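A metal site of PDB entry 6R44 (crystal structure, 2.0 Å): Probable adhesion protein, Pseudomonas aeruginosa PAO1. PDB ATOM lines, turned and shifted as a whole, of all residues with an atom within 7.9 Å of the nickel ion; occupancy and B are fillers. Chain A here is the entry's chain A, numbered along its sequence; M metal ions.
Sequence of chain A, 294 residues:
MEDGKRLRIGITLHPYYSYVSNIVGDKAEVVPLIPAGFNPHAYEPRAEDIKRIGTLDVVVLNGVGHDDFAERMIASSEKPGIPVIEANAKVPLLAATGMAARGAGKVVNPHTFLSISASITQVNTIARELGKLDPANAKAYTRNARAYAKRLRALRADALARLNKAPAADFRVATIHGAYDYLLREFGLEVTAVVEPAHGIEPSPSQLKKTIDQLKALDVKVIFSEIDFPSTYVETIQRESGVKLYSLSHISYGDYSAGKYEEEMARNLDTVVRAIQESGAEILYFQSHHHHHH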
ATOM      1  N   LEU A  13       4.233  25.160 -18.946  1.00  0.00           N
ATOM      2  CA  LEU A  13       3.527  23.892 -19.220  1.00  0.00           C
ATOM      3  C   LEU A  13       3.666  22.944 -18.041  1.00  0.00           C
ATOM      4  O   LEU A  13       4.632  23.044 -17.291  1.00  0.00           O
ATOM      5  CB  LEU A  13       4.023  23.258 -20.529  1.00  0.00           C
ATOM      6  CG  LEU A  13       3.984  24.139 -21.816  1.00  0.00           C
ATOM      7  CD1 LEU A  13       4.865  23.536 -22.914  1.00  0.00           C
ATOM      8  CD2 LEU A  13       2.538  24.320 -22.346  1.00  0.00           C
ATOM      9  N   ASN A  39      -6.298  25.492 -22.024  1.00  0.00           N
ATOM     10  CA  ASN A  39      -5.628  24.573 -22.935  1.00  0.00           C
ATOM     11  C   ASN A  39      -4.452  25.440 -23.456  1.00  0.00           C
ATOM     12  O   ASN A  39      -4.704  26.542 -23.961  1.00  0.00           O
ATOM     13  CB  ASN A  39      -6.547  24.133 -24.091  1.00  0.00           C
ATOM     14  CG  ASN A  39      -5.874  23.207 -25.089  1.00  0.00           C
ATOM     15  OD1 ASN A  39      -4.661  23.213 -25.281  1.00  0.00           O
ATOM     16  ND2 ASN A  39      -6.643  22.384 -25.770  1.00  0.00           N
ATOM     17  N   PRO A  40      -3.174  25.027 -23.277  1.00  0.00           N
ATOM     18  CA  PRO A  40      -2.074  25.908 -23.697  1.00  0.00           C
ATOM     19  C   PRO A  40      -1.990  26.121 -25.206  1.00  0.00           C
ATOM     20  O   PRO A  40      -1.384  27.072 -25.658  1.00  0.00           O
ATOM     21  CB  PRO A  40      -0.847  25.210 -23.115  1.00  0.00           C
ATOM     22  CG  PRO A  40      -1.232  23.760 -23.065  1.00  0.00           C
ATOM     23  CD  PRO A  40      -2.658  23.798 -22.639  1.00  0.00           C
ATOM     24  N   HIS A  41      -2.651  25.266 -25.993  1.00  0.00           N
ATOM     25  CA  HIS A  41      -2.680  25.436 -27.443  1.00  0.00           C
ATOM     26  C   HIS A  41      -3.617  26.586 -27.827  1.00  0.00           C
ATOM     27  O   HIS A  41      -3.383  27.222 -28.832  1.00  0.00           O
ATOM     28  CB  HIS A  41      -3.177  24.148 -28.110  1.00  0.00           C
ATOM     29  CG  HIS A  41      -2.278  22.977 -27.853  1.00  0.00           C
ATOM     30  ND1 HIS A  41      -2.482  22.144 -26.780  1.00  0.00           N
ATOM     31  CD2 HIS A  41      -1.170  22.579 -28.520  1.00  0.00           C
ATOM     32  CE1 HIS A  41      -1.518  21.228 -26.843  1.00  0.00           C
ATOM     33  NE2 HIS A  41      -0.696  21.455 -27.857  1.00  0.00           N
ATOM     34  N   GLY A  65       8.831  26.212 -29.534  1.00  0.00           N
ATOM     35  CA  GLY A  65       7.550  26.252 -30.222  1.00  0.00           C
ATOM     36  C   GLY A  65       6.314  25.890 -29.407  1.00  0.00           C
ATOM     37  O   GLY A  65       5.208  26.028 -29.924  1.00  0.00           O
ATOM     38  N   HIS A  66       6.482  25.416 -28.136  1.00  0.00           N
ATOM     39  CA  HIS A  66       5.298  25.075 -27.355  1.00  0.00           C
ATOM     40  C   HIS A  66       4.894  26.145 -26.310  1.00  0.00           C
ATOM     41  O   HIS A  66       3.951  25.938 -25.538  1.00  0.00           O
ATOM     42  CB  HIS A  66       5.376  23.680 -26.705  1.00  0.00           C
ATOM     43  CG  HIS A  66       4.073  22.942 -26.789  1.00  0.00           C
ATOM     44  ND1 HIS A  66       2.895  23.504 -26.299  1.00  0.00           N
ATOM     45  CD2 HIS A  66       3.777  21.775 -27.412  1.00  0.00           C
ATOM     46  CE1 HIS A  66       1.935  22.628 -26.582  1.00  0.00           C
ATOM     47  NE2 HIS A  66       2.419  21.578 -27.273  1.00  0.00           N
ATOM     48  N   ASN A 109       9.547  19.929 -33.910  1.00  0.00           N
ATOM     49  CA  ASN A 109       8.512  19.353 -33.055  1.00  0.00           C
ATOM     50  C   ASN A 109       8.829  19.819 -31.610  1.00  0.00           C
ATOM     51  O   ASN A 109       9.870  19.468 -31.072  1.00  0.00           O
ATOM     52  CB  ASN A 109       8.459  17.840 -33.163  1.00  0.00           C
ATOM     53  CG  ASN A 109       7.276  17.261 -32.422  1.00  0.00           C
ATOM     54  OD1 ASN A 109       6.940  17.666 -31.316  1.00  0.00           O
ATOM     55  ND2 ASN A 109       6.615  16.292 -33.019  1.00  0.00           N
ATOM     56  N   PRO A 110       7.967  20.640 -30.987  1.00  0.00           N
ATOM     57  CA  PRO A 110       8.337  21.192 -29.664  1.00  0.00           C
ATOM     58  C   PRO A 110       8.079  20.311 -28.443  1.00  0.00           C
ATOM     59  O   PRO A 110       8.415  20.713 -27.342  1.00  0.00           O
ATOM     60  CB  PRO A 110       7.489  22.460 -29.608  1.00  0.00           C
ATOM     61  CG  PRO A 110       6.204  22.059 -30.303  1.00  0.00           C
ATOM     62  CD  PRO A 110       6.699  21.228 -31.481  1.00  0.00           C
ATOM     63  N   HIS A 111       7.474  19.111 -28.633  1.00  0.00           N
ATOM     64  CA  HIS A 111       7.041  18.182 -27.594  1.00  0.00           C
ATOM     65  C   HIS A 111       8.176  17.314 -27.006  1.00  0.00           C
ATOM     66  O   HIS A 111       8.000  16.087 -26.776  1.00  0.00           O
ATOM     67  CB  HIS A 111       5.885  17.305 -28.120  1.00  0.00           C
ATOM     68  CG  HIS A 111       4.716  18.082 -28.631  1.00  0.00           C
ATOM     69  ND1 HIS A 111       4.655  18.509 -29.929  1.00  0.00           N
ATOM     70  CD2 HIS A 111       3.552  18.396 -28.011  1.00  0.00           C
ATOM     71  CE1 HIS A 111       3.477  19.108 -30.068  1.00  0.00           C
ATOM     72  NE2 HIS A 111       2.793  19.106 -28.929  1.00  0.00           N
ATOM     73  N   PHE A 113       9.318  17.375 -24.024  1.00  0.00           N
ATOM     74  CA  PHE A 113       8.912  16.980 -22.672  1.00  0.00           C
ATOM     75  C   PHE A 113       8.177  15.629 -22.662  1.00  0.00           C
ATOM     76  O   PHE A 113       8.062  15.021 -21.610  1.00  0.00           O
ATOM     77  CB  PHE A 113       8.053  18.083 -21.995  1.00  0.00           C
ATOM     78  CG  PHE A 113       6.938  18.636 -22.852  1.00  0.00           C
ATOM     79  CD1 PHE A 113       5.695  17.987 -22.918  1.00  0.00           C
ATOM     80  CD2 PHE A 113       7.121  19.786 -23.621  1.00  0.00           C
ATOM     81  CE1 PHE A 113       4.676  18.485 -23.745  1.00  0.00           C
ATOM     82  CE2 PHE A 113       6.102  20.285 -24.431  1.00  0.00           C
ATOM     83  CZ  PHE A 113       4.879  19.628 -24.484  1.00  0.00           C
ATOM     84  N   LEU A 114       7.738  15.110 -23.822  1.00  0.00           N
ATOM     85  CA  LEU A 114       7.068  13.819 -23.798  1.00  0.00           C
ATOM     86  C   LEU A 114       8.047  12.636 -23.984  1.00  0.00           C
ATOM     87  O   LEU A 114       7.620  11.509 -24.139  1.00  0.00           O
ATOM     88  CB  LEU A 114       5.863  13.761 -24.754  1.00  0.00           C
ATOM     89  CG  LEU A 114       4.740  14.738 -24.359  1.00  0.00           C
ATOM     90  CD1 LEU A 114       3.598  14.694 -25.333  1.00  0.00           C
ATOM     91  CD2 LEU A 114       4.223  14.465 -22.927  1.00  0.00           C
ATOM     92  N   HIS A 177      -2.559  14.425 -32.515  1.00  0.00           N
ATOM     93  CA  HIS A 177      -1.685  15.566 -32.214  1.00  0.00           C
ATOM     94  C   HIS A 177      -0.274  15.112 -32.521  1.00  0.00           C
ATOM     95  O   HIS A 177       0.051  13.950 -32.258  1.00  0.00           O
ATOM     96  CB  HIS A 177      -1.776  15.889 -30.701  1.00  0.00           C
ATOM     97  CG  HIS A 177      -1.327  17.260 -30.309  1.00  0.00           C
ATOM     98  ND1 HIS A 177      -2.214  18.311 -30.249  1.00  0.00           N
ATOM     99  CD2 HIS A 177      -0.116  17.697 -29.880  1.00  0.00           C
ATOM    100  CE1 HIS A 177      -1.512  19.355 -29.842  1.00  0.00           C
ATOM    101  NE2 HIS A 177      -0.263  19.023 -29.560  1.00  0.00           N
ATOM    102  N   GLY A 178       0.572  16.018 -33.002  1.00  0.00           N
ATOM    103  CA  GLY A 178       1.972  15.686 -33.296  1.00  0.00           C
ATOM    104  C   GLY A 178       2.845  15.760 -32.060  1.00  0.00           C
ATOM    105  O   GLY A 178       3.926  16.351 -32.098  1.00  0.00           O
ATOM    106  N   ALA A 179       2.402  15.156 -30.959  1.00  0.00           N
ATOM    107  CA  ALA A 179       3.083  15.172 -29.672  1.00  0.00           C
ATOM    108  C   ALA A 179       4.048  14.062 -29.384  1.00  0.00           C
ATOM    109  O   ALA A 179       4.847  14.237 -28.482  1.00  0.00           O
ATOM    110  CB  ALA A 179       2.044  15.178 -28.561  1.00  0.00           C
ATOM    111  N   GLU A 196      -3.673  15.981 -37.240  1.00  0.00           N
ATOM    112  CA  GLU A 196      -3.701  17.447 -37.280  1.00  0.00           C
ATOM    113  C   GLU A 196      -2.702  17.946 -38.357  1.00  0.00           C
ATOM    114  O   GLU A 196      -1.538  17.524 -38.331  1.00  0.00           O
ATOM    115  CB  GLU A 196      -3.361  18.047 -35.921  1.00  0.00           C
ATOM    116  CG  GLU A 196      -4.476  17.845 -34.918  1.00  0.00           C
ATOM    117  CD  GLU A 196      -4.342  18.601 -33.612  1.00  0.00           C
ATOM    118  OE1 GLU A 196      -3.214  18.999 -33.246  1.00  0.00           O
ATOM    119  OE2 GLU A 196      -5.390  18.801 -32.956  1.00  0.00           O
ATOM    120  N   HIS A 199       0.589  21.859 -35.853  1.00  0.00           N
ATOM    121  CA  HIS A 199       0.446  21.841 -34.384  1.00  0.00           C
ATOM    122  C   HIS A 199      -0.814  22.561 -33.868  1.00  0.00           C
ATOM    123  O   HIS A 199      -0.994  23.746 -34.134  1.00  0.00           O
ATOM    124  CB  HIS A 199       1.709  22.372 -33.694  1.00  0.00           C
ATOM    125  CG  HIS A 199       1.660  22.219 -32.200  1.00  0.00           C
ATOM    126  ND1 HIS A 199       2.168  23.184 -31.358  1.00  0.00           N
ATOM    127  CD2 HIS A 199       1.153  21.210 -31.458  1.00  0.00           C
ATOM    128  CE1 HIS A 199       1.971  22.725 -30.134  1.00  0.00           C
ATOM    129  NE2 HIS A 199       1.364  21.533 -30.145  1.00  0.00           N
ATOM    130  N   GLY A 200      -1.686  21.815 -33.185  1.00  0.00           N
ATOM    131  CA  GLY A 200      -2.937  22.366 -32.639  1.00  0.00           C
ATOM    132  C   GLY A 200      -3.934  22.881 -33.675  1.00  0.00           C
ATOM    133  O   GLY A 200      -4.860  23.618 -33.313  1.00  0.00           O
ATOM    134  N   GLU A 226      -5.954  11.788 -28.274  1.00  0.00           N
ATOM    135  CA  GLU A 226      -5.720  12.646 -27.112  1.00  0.00           C
ATOM    136  C   GLU A 226      -6.644  12.355 -25.928  1.00  0.00           C
ATOM    137  O   GLU A 226      -7.858  12.280 -26.090  1.00  0.00           O
ATOM    138  CB  GLU A 226      -5.860  14.126 -27.563  1.00  0.00           C
ATOM    139  CG  GLU A 226      -4.700  14.619 -28.431  1.00  0.00           C
ATOM    140  CD  GLU A 226      -3.373  14.564 -27.706  1.00  0.00           C
ATOM    141  OE1 GLU A 226      -3.134  15.421 -26.827  1.00  0.00           O
ATOM    142  OE2 GLU A 226      -2.581  13.646 -27.993  1.00  0.00           O
ATOM    143  N   HIS A 250      -0.927  14.378 -23.351  1.00  0.00           N
ATOM    144  CA  HIS A 250      -0.036  15.488 -23.714  1.00  0.00           C
ATOM    145  C   HIS A 250       0.495  16.147 -22.389  1.00  0.00           C
ATOM    146  O   HIS A 250       1.382  16.989 -22.447  1.00  0.00           O
ATOM    147  CB  HIS A 250      -0.828  16.522 -24.531  1.00  0.00           C
ATOM    148  CG  HIS A 250      -0.026  17.619 -25.173  1.00  0.00           C
ATOM    149  ND1 HIS A 250       0.722  18.522 -24.411  1.00  0.00           N
ATOM    150  CD2 HIS A 250       0.051  17.984 -26.468  1.00  0.00           C
ATOM    151  CE1 HIS A 250       1.290  19.332 -25.276  1.00  0.00           C
ATOM    152  NE2 HIS A 250       0.878  19.090 -26.508  1.00  0.00           N
ATOM    153  N   SER A 252      -1.152  18.142 -20.351  1.00  0.00           N
ATOM    154  CA  SER A 252      -1.551  19.532 -20.517  1.00  0.00           C
ATOM    155  C   SER A 252      -2.858  19.838 -19.802  1.00  0.00           C
ATOM    156  O   SER A 252      -3.373  20.923 -19.989  1.00  0.00           O
ATOM    157  CB  SER A 252      -1.728  19.820 -21.999  1.00  0.00           C
ATOM    158  OG  SER A 252      -2.804  19.022 -22.512  1.00  0.00           O
HETATM  159 NI    NI M   1       1.011  20.277 -28.440  1.00  0.00          NI
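OD1 of Asn 109 is in hydrogen-bond range of ND1 of His 111, at 2.8 Å. ND1 of His 41 is in hydrogen-bond range of OD1 of Asn 39, at 2.9 Å. The side-chain carboxylate of Glu 196 is in hydrogen-bond range of a ring nitrogen (ND1) of His 177, 3.2 Å away. A ring nitrogen (ND1) of His 111 lies within hydrogen-bond range of the backbone carbonyl oxygen (O) of Gly 178, at 3.1 Å.
Of the 20 residues printed, 6 come within 4 Å of the nickel ion. The nearest printed residue that does not touch the nickel ion is Ala 179 (5.2 Å).
The nickel ion is bound by NE2 of His 177 (2.1 Å), NE2 of His 199 (2.1 Å), NE2 of His 41 (2.2 Å), NE2 of His 111 (2.2 Å), NE2 of His 66 (2.2 Å) and NE2 of His 250 (2.3 Å). The nickel ion has six donor atoms within binding distance.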
